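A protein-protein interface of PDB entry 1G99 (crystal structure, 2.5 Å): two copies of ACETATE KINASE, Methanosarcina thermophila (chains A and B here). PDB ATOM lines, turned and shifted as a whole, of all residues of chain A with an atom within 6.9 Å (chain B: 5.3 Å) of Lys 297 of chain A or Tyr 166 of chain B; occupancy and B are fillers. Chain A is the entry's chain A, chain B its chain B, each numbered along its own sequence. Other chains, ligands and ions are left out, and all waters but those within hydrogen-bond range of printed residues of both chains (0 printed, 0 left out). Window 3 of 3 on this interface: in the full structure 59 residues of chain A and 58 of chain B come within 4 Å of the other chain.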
ATOM      1  N   LYS A 271       9.527  24.892 -24.683  1.00  0.00           N
ATOM      2  CA  LYS A 271      10.875  24.471 -24.373  1.00  0.00           C
ATOM      3  C   LYS A 271      11.699  25.537 -23.690  1.00  0.00           C
ATOM      4  O   LYS A 271      12.893  25.376 -23.506  1.00  0.00           O
ATOM      5  CB  LYS A 271      11.555  24.044 -25.671  1.00  0.00           C
ATOM      6  CG  LYS A 271      10.922  22.848 -26.320  1.00  0.00           C
ATOM      7  CD  LYS A 271      11.415  22.758 -27.749  1.00  0.00           C
ATOM      8  CE  LYS A 271      10.970  21.478 -28.437  1.00  0.00           C
ATOM      9  NZ  LYS A 271      11.456  21.460 -29.840  1.00  0.00           N
ATOM     10  N   VAL A 274      11.957  28.265 -17.116  1.00  0.00           N
ATOM     11  CA  VAL A 274      12.938  27.619 -16.245  1.00  0.00           C
ATOM     12  C   VAL A 274      13.294  26.207 -16.762  1.00  0.00           C
ATOM     13  O   VAL A 274      14.364  25.671 -16.452  1.00  0.00           O
ATOM     14  CB  VAL A 274      12.448  27.574 -14.781  1.00  0.00           C
ATOM     15  CG1 VAL A 274      12.367  28.968 -14.247  1.00  0.00           C
ATOM     16  CG2 VAL A 274      11.079  26.875 -14.686  1.00  0.00           C
ATOM     17  N   LEU A 275      12.418  25.613 -17.575  1.00  0.00           N
ATOM     18  CA  LEU A 275      12.709  24.282 -18.129  1.00  0.00           C
ATOM     19  C   LEU A 275      13.884  24.404 -19.104  1.00  0.00           C
ATOM     20  O   LEU A 275      14.858  23.652 -19.039  1.00  0.00           O
ATOM     21  CB  LEU A 275      11.496  23.710 -18.866  1.00  0.00           C
ATOM     22  CG  LEU A 275      11.793  22.476 -19.754  1.00  0.00           C
ATOM     23  CD1 LEU A 275      12.111  21.304 -18.865  1.00  0.00           C
ATOM     24  CD2 LEU A 275      10.609  22.118 -20.657  1.00  0.00           C
ATOM     25  N   GLY A 276      13.795  25.379 -20.001  1.00  0.00           N
ATOM     26  CA  GLY A 276      14.849  25.592 -20.967  1.00  0.00           C
ATOM     27  C   GLY A 276      16.206  25.964 -20.383  1.00  0.00           C
ATOM     28  O   GLY A 276      17.248  25.523 -20.875  1.00  0.00           O
ATOM     29  N   VAL A 277      16.208  26.776 -19.338  1.00  0.00           N
ATOM     30  CA  VAL A 277      17.450  27.199 -18.706  1.00  0.00           C
ATOM     31  C   VAL A 277      18.066  26.075 -17.869  1.00  0.00           C
ATOM     32  O   VAL A 277      19.266  25.801 -17.963  1.00  0.00           O
ATOM     33  CB  VAL A 277      17.220  28.423 -17.760  1.00  0.00           C
ATOM     34  CG1 VAL A 277      18.495  28.721 -16.983  1.00  0.00           C
ATOM     35  CG2 VAL A 277      16.753  29.649 -18.561  1.00  0.00           C
ATOM     36  N   SER A 278      17.246  25.437 -17.047  1.00  0.00           N
ATOM     37  CA  SER A 278      17.722  24.382 -16.163  1.00  0.00           C
ATOM     38  C   SER A 278      18.086  23.096 -16.878  1.00  0.00           C
ATOM     39  O   SER A 278      18.991  22.394 -16.455  1.00  0.00           O
ATOM     40  CB  SER A 278      16.665  24.057 -15.090  1.00  0.00           C
ATOM     41  OG  SER A 278      15.528  23.384 -15.648  1.00  0.00           O
ATOM     42  N   GLY A 279      17.381  22.787 -17.965  1.00  0.00           N
ATOM     43  CA  GLY A 279      17.633  21.543 -18.664  1.00  0.00           C
ATOM     44  C   GLY A 279      17.089  20.427 -17.802  1.00  0.00           C
ATOM     45  O   GLY A 279      17.224  19.257 -18.115  1.00  0.00           O
ATOM     46  N   LEU A 280      16.413  20.790 -16.723  1.00  0.00           N
ATOM     47  CA  LEU A 280      15.911  19.803 -15.783  1.00  0.00           C
ATOM     48  C   LEU A 280      14.399  19.633 -15.652  1.00  0.00           C
ATOM     49  O   LEU A 280      13.874  18.552 -15.857  1.00  0.00           O
ATOM     50  CB  LEU A 280      16.472  20.112 -14.398  1.00  0.00           C
ATOM     51  CG  LEU A 280      16.236  19.052 -13.330  1.00  0.00           C
ATOM     52  CD1 LEU A 280      17.193  17.921 -13.577  1.00  0.00           C
ATOM     53  CD2 LEU A 280      16.464  19.639 -11.962  1.00  0.00           C
ATOM     54  N   LEU A 287      13.163  22.207  -9.006  1.00  0.00           N
ATOM     55  CA  LEU A 287      14.310  23.096  -9.205  1.00  0.00           C
ATOM     56  C   LEU A 287      14.886  23.565  -7.881  1.00  0.00           C
ATOM     57  O   LEU A 287      16.099  23.620  -7.706  1.00  0.00           O
ATOM     58  CB  LEU A 287      13.918  24.308 -10.068  1.00  0.00           C
ATOM     59  CG  LEU A 287      13.469  23.964 -11.496  1.00  0.00           C
ATOM     60  CD1 LEU A 287      13.174  25.231 -12.251  1.00  0.00           C
ATOM     61  CD2 LEU A 287      14.536  23.194 -12.226  1.00  0.00           C
ATOM     62  N   GLY A 294      23.098  21.848  -5.069  1.00  0.00           N
ATOM     63  CA  GLY A 294      24.189  22.330  -5.909  1.00  0.00           C
ATOM     64  C   GLY A 294      24.095  22.330  -7.440  1.00  0.00           C
ATOM     65  O   GLY A 294      25.109  22.514  -8.121  1.00  0.00           O
ATOM     66  N   ASN A 295      22.905  22.132  -7.997  1.00  0.00           N
ATOM     67  CA  ASN A 295      22.730  22.122  -9.454  1.00  0.00           C
ATOM     68  C   ASN A 295      22.687  23.572  -9.971  1.00  0.00           C
ATOM     69  O   ASN A 295      21.682  24.264  -9.801  1.00  0.00           O
ATOM     70  CB  ASN A 295      21.423  21.417  -9.813  1.00  0.00           C
ATOM     71  CG  ASN A 295      21.183  21.378 -11.307  1.00  0.00           C
ATOM     72  OD1 ASN A 295      21.536  22.300 -12.030  1.00  0.00           O
ATOM     73  ND2 ASN A 295      20.565  20.316 -11.774  1.00  0.00           N
ATOM     74  N   ARG A 296      23.766  24.003 -10.624  1.00  0.00           N
ATOM     75  CA  ARG A 296      23.907  25.368 -11.109  1.00  0.00           C
ATOM     76  C   ARG A 296      22.843  25.857 -12.101  1.00  0.00           C
ATOM     77  O   ARG A 296      22.333  26.968 -11.968  1.00  0.00           O
ATOM     78  CB  ARG A 296      25.316  25.546 -11.686  1.00  0.00           C
ATOM     79  CG  ARG A 296      25.574  26.905 -12.266  1.00  0.00           C
ATOM     80  CD  ARG A 296      25.208  28.015 -11.297  1.00  0.00           C
ATOM     81  NE  ARG A 296      25.343  29.312 -11.956  1.00  0.00           N
ATOM     82  CZ  ARG A 296      24.922  30.463 -11.444  1.00  0.00           C
ATOM     83  NH1 ARG A 296      24.323  30.500 -10.257  1.00  0.00           N
ATOM     84  NH2 ARG A 296      25.129  31.585 -12.109  1.00  0.00           N
ATOM     85  N   LYS A 297      22.514  25.040 -13.089  1.00  0.00           N
ATOM     86  CA  LYS A 297      21.510  25.426 -14.058  1.00  0.00           C
ATOM     87  C   LYS A 297      20.167  25.660 -13.361  1.00  0.00           C
ATOM     88  O   LYS A 297      19.440  26.577 -13.721  1.00  0.00           O
ATOM     89  CB  LYS A 297      21.322  24.346 -15.113  1.00  0.00           C
ATOM     90  CG  LYS A 297      22.506  24.069 -15.968  1.00  0.00           C
ATOM     91  CD  LYS A 297      22.881  25.223 -16.803  1.00  0.00           C
ATOM     92  CE  LYS A 297      23.861  24.769 -17.870  1.00  0.00           C
ATOM     93  NZ  LYS A 297      23.299  23.677 -18.681  1.00  0.00           N
ATOM     94  N   ALA A 298      19.840  24.824 -12.377  1.00  0.00           N
ATOM     95  CA  ALA A 298      18.599  24.970 -11.643  1.00  0.00           C
ATOM     96  C   ALA A 298      18.635  26.261 -10.830  1.00  0.00           C
ATOM     97  O   ALA A 298      17.645  26.972 -10.763  1.00  0.00           O
ATOM     98  CB  ALA A 298      18.385  23.760 -10.716  1.00  0.00           C
ATOM     99  N   GLU A 299      19.787  26.550 -10.232  1.00  0.00           N
ATOM    100  CA  GLU A 299      19.973  27.748  -9.435  1.00  0.00           C
ATOM    101  C   GLU A 299      19.816  28.982 -10.342  1.00  0.00           C
ATOM    102  O   GLU A 299      19.094  29.915  -9.977  1.00  0.00           O
ATOM    103  CB  GLU A 299      21.359  27.709  -8.746  1.00  0.00           C
ATOM    104  CG  GLU A 299      21.821  28.953  -7.932  1.00  0.00           C
ATOM    105  CD  GLU A 299      20.795  29.445  -6.878  1.00  0.00           C
ATOM    106  OE1 GLU A 299      20.101  28.597  -6.245  1.00  0.00           O
ATOM    107  OE2 GLU A 299      20.700  30.697  -6.664  1.00  0.00           O
ATOM    108  N   LEU A 300      20.455  28.973 -11.518  1.00  0.00           N
ATOM    109  CA  LEU A 300      20.363  30.102 -12.449  1.00  0.00           C
ATOM    110  C   LEU A 300      18.905  30.325 -12.893  1.00  0.00           C
ATOM    111  O   LEU A 300      18.443  31.456 -12.965  1.00  0.00           O
ATOM    112  CB  LEU A 300      21.258  29.855 -13.670  1.00  0.00           C
ATOM    113  CG  LEU A 300      21.277  30.889 -14.796  1.00  0.00           C
ATOM    114  CD1 LEU A 300      21.656  32.282 -14.271  1.00  0.00           C
ATOM    115  CD2 LEU A 300      22.260  30.434 -15.834  1.00  0.00           C
ATOM    116  N   ALA A 301      18.175  29.244 -13.141  1.00  0.00           N
ATOM    117  CA  ALA A 301      16.789  29.354 -13.569  1.00  0.00           C
ATOM    118  C   ALA A 301      15.936  30.030 -12.495  1.00  0.00           C
ATOM    119  O   ALA A 301      15.104  30.881 -12.813  1.00  0.00           O
ATOM    120  CB  ALA A 301      16.233  27.970 -13.902  1.00  0.00           C
ATOM    121  N   LEU A 302      16.126  29.659 -11.226  1.00  0.00           N
ATOM    122  CA  LEU A 302      15.371  30.303 -10.158  1.00  0.00           C
ATOM    123  C   LEU A 302      15.781  31.769  -9.967  1.00  0.00           C
ATOM    124  O   LEU A 302      14.952  32.587  -9.600  1.00  0.00           O
ATOM    125  CB  LEU A 302      15.533  29.554  -8.842  1.00  0.00           C
ATOM    126  CG  LEU A 302      14.910  28.174  -8.821  1.00  0.00           C
ATOM    127  CD1 LEU A 302      15.293  27.485  -7.523  1.00  0.00           C
ATOM    128  CD2 LEU A 302      13.395  28.284  -8.998  1.00  0.00           C
ATOM    129  N   MET B 161      21.125  36.701 -19.242  1.00  0.00           N
ATOM    130  CA  MET B 161      20.646  35.464 -19.842  1.00  0.00           C
ATOM    131  C   MET B 161      19.138  35.563 -20.091  1.00  0.00           C
ATOM    132  O   MET B 161      18.414  36.092 -19.256  1.00  0.00           O
ATOM    133  CB  MET B 161      20.871  34.270 -18.905  1.00  0.00           C
ATOM    134  CG  MET B 161      22.310  33.852 -18.688  1.00  0.00           C
ATOM    135  SD  MET B 161      23.111  33.089 -20.127  1.00  0.00           S
ATOM    136  CE  MET B 161      21.981  31.709 -20.431  1.00  0.00           C
ATOM    137  N   LEU B 164      15.597  31.133 -22.242  1.00  0.00           N
ATOM    138  CA  LEU B 164      15.486  30.309 -23.439  1.00  0.00           C
ATOM    139  C   LEU B 164      16.308  29.059 -23.187  1.00  0.00           C
ATOM    140  O   LEU B 164      16.997  28.958 -22.166  1.00  0.00           O
ATOM    141  CB  LEU B 164      16.058  31.053 -24.646  1.00  0.00           C
ATOM    142  CG  LEU B 164      15.168  32.171 -25.192  1.00  0.00           C
ATOM    143  CD1 LEU B 164      15.998  33.032 -26.122  1.00  0.00           C
ATOM    144  CD2 LEU B 164      13.958  31.579 -25.890  1.00  0.00           C
ATOM    145  N   PRO B 165      16.241  28.080 -24.104  1.00  0.00           N
ATOM    146  CA  PRO B 165      17.033  26.854 -23.905  1.00  0.00           C
ATOM    147  C   PRO B 165      18.486  27.297 -23.785  1.00  0.00           C
ATOM    148  O   PRO B 165      18.971  28.085 -24.598  1.00  0.00           O
ATOM    149  CB  PRO B 165      16.767  26.055 -25.177  1.00  0.00           C
ATOM    150  CG  PRO B 165      15.350  26.471 -25.549  1.00  0.00           C
ATOM    151  CD  PRO B 165      15.401  27.988 -25.310  1.00  0.00           C
ATOM    152  N   TYR B 166      19.174  26.815 -22.759  1.00  0.00           N
ATOM    153  CA  TYR B 166      20.560  27.189 -22.502  1.00  0.00           C
ATOM    154  C   TYR B 166      21.536  27.008 -23.686  1.00  0.00           C
ATOM    155  O   TYR B 166      22.468  27.801 -23.872  1.00  0.00           O
ATOM    156  CB  TYR B 166      21.069  26.399 -21.311  1.00  0.00           C
ATOM    157  CG  TYR B 166      22.342  26.956 -20.730  1.00  0.00           C
ATOM    158  CD1 TYR B 166      22.309  27.987 -19.786  1.00  0.00           C
ATOM    159  CD2 TYR B 166      23.589  26.496 -21.163  1.00  0.00           C
ATOM    160  CE1 TYR B 166      23.496  28.554 -19.287  1.00  0.00           C
ATOM    161  CE2 TYR B 166      24.784  27.059 -20.682  1.00  0.00           C
ATOM    162  CZ  TYR B 166      24.730  28.085 -19.749  1.00  0.00           C
ATOM    163  OH  TYR B 166      25.902  28.667 -19.327  1.00  0.00           O
ATOM    164  N   ASP B 167      21.337  25.971 -24.487  1.00  0.00           N
ATOM    165  CA  ASP B 167      22.244  25.715 -25.605  1.00  0.00           C
ATOM    166  C   ASP B 167      22.294  26.854 -26.623  1.00  0.00           C
ATOM    167  O   ASP B 167      23.297  27.029 -27.300  1.00  0.00           O
ATOM    168  CB  ASP B 167      21.899  24.375 -26.290  1.00  0.00           C
ATOM    169  CG  ASP B 167      20.602  24.422 -27.076  1.00  0.00           C
ATOM    170  OD1 ASP B 167      19.584  24.933 -26.565  1.00  0.00           O
ATOM    171  OD2 ASP B 167      20.601  23.929 -28.222  1.00  0.00           O
ATOM    172  N   LEU B 168      21.227  27.639 -26.726  1.00  0.00           N
ATOM    173  CA  LEU B 168      21.219  28.739 -27.682  1.00  0.00           C
ATOM    174  C   LEU B 168      22.225  29.775 -27.250  1.00  0.00           C
ATOM    175  O   LEU B 168      22.829  30.463 -28.079  1.00  0.00           O
ATOM    176  CB  LEU B 168      19.826  29.381 -27.777  1.00  0.00           C
ATOM    177  CG  LEU B 168      18.725  28.428 -28.275  1.00  0.00           C
ATOM    178  CD1 LEU B 168      17.471  29.225 -28.485  1.00  0.00           C
ATOM    179  CD2 LEU B 168      19.146  27.716 -29.581  1.00  0.00           C
ATOM    180  N   TYR B 169      22.409  29.895 -25.937  1.00  0.00           N
ATOM    181  CA  TYR B 169      23.368  30.849 -25.412  1.00  0.00           C
ATOM    182  C   TYR B 169      24.764  30.348 -25.769  1.00  0.00           C
ATOM    183  O   TYR B 169      25.626  31.091 -26.211  1.00  0.00           O
ATOM    184  CB  TYR B 169      23.265  30.956 -23.889  1.00  0.00           C
ATOM    185  CG  TYR B 169      24.519  31.561 -23.270  1.00  0.00           C
ATOM    186  CD1 TYR B 169      24.907  32.854 -23.592  1.00  0.00           C
ATOM    187  CD2 TYR B 169      25.331  30.820 -22.406  1.00  0.00           C
ATOM    188  CE1 TYR B 169      26.052  33.403 -23.090  1.00  0.00           C
ATOM    189  CE2 TYR B 169      26.507  31.368 -21.885  1.00  0.00           C
ATOM    190  CZ  TYR B 169      26.856  32.667 -22.241  1.00  0.00           C
ATOM    191  OH  TYR B 169      28.022  33.248 -21.784  1.00  0.00           O
ATOM    192  N   GLU B 170      24.974  29.063 -25.587  1.00  0.00           N
ATOM    193  CA  GLU B 170      26.269  28.481 -25.867  1.00  0.00           C
ATOM    194  C   GLU B 170      26.603  28.322 -27.358  1.00  0.00           C
ATOM    195  O   GLU B 170      27.724  28.573 -27.763  1.00  0.00           O
ATOM    196  CB  GLU B 170      26.357  27.144 -25.165  1.00  0.00           C
ATOM    197  CG  GLU B 170      27.708  26.866 -24.667  1.00  0.00           C
ATOM    198  CD  GLU B 170      27.647  26.103 -23.384  1.00  0.00           C
ATOM    199  OE1 GLU B 170      26.875  25.111 -23.349  1.00  0.00           O
ATOM    200  OE2 GLU B 170      28.359  26.495 -22.427  1.00  0.00           O
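Printed residues of chain B within 4 Å of Lys 271 of chain A: Pro 165.
Printed residues of chain B within 4 Å of Gly 276 of chain A: Leu 164, Pro 165 and Tyr 166.
Of the printed residues of chain B, Val 277 of chain A touches Leu 164 and Tyr 166.
Gly 294 of chain A touches none of the printed residues of chain B.
Lys 297 of chain A touches just one residue of chain B: Tyr 166 (3.7 Å).
Met 161 of chain B touches none of the printed residues of chain A.
Of the printed residues of chain A, Leu 164 of chain B touches Gly 276 and Val 277.
Of the printed residues of chain A, Pro 165 of chain B touches Lys 271 and Gly 276.
Printed residues of chain A within 4 Å of Tyr 166 of chain B: Gly 276 (3.0 Å), Val 277 (3.8 Å) and Lys 297 (3.7 Å).
The nearest printed residue of chain B that does not touch Lys 297 of chain A is Glu 170 of chain B (6.1 Å).
The nearest residue of chain A that does not touch Tyr 166 of chain B is Leu 300 of chain A (4.1 Å).
Among the printed residues, merely in contact across the chains: Lys 271 of chain A with Pro 165 of chain B, Gly 276 of chain A with Leu 164 of chain B, Gly 276 of chain A with Pro 165 of chain B, Val 277 of chain A with Leu 164 of chain B, Val 277 of chain A with Tyr 166 of chain B and Lys 297 of chain A with Tyr 166 of chain B.
The backbone NH (N) of Lys 297 of chain A is in hydrogen-bond range of the side-chain amide oxygen (OD1) of Asn 295 of chain A.
Of the 18 printed residues of chain A, 4 touch a printed residue of chain B.
Hydrophobic or aromatic side chains of chain A that line the printed part of chain B: Val 277.
Of the 8 printed residues of chain B, 3 touch a printed residue of chain A.
Hydrophobic or aromatic side chains of chain B that line the printed part of chain A: Pro 165 and Tyr 166.
Among the printed residues, 7 pairs touch across the chains.
No position is printed for both chains.
Of the 7 pairs that touch across the chains among the printed residues, none has its exchanged pair printed and touching as well.
O of Gly 276 of chain A lies within hydrogen-bond range of N of Tyr 166 of chain B, 3.0 Å away.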
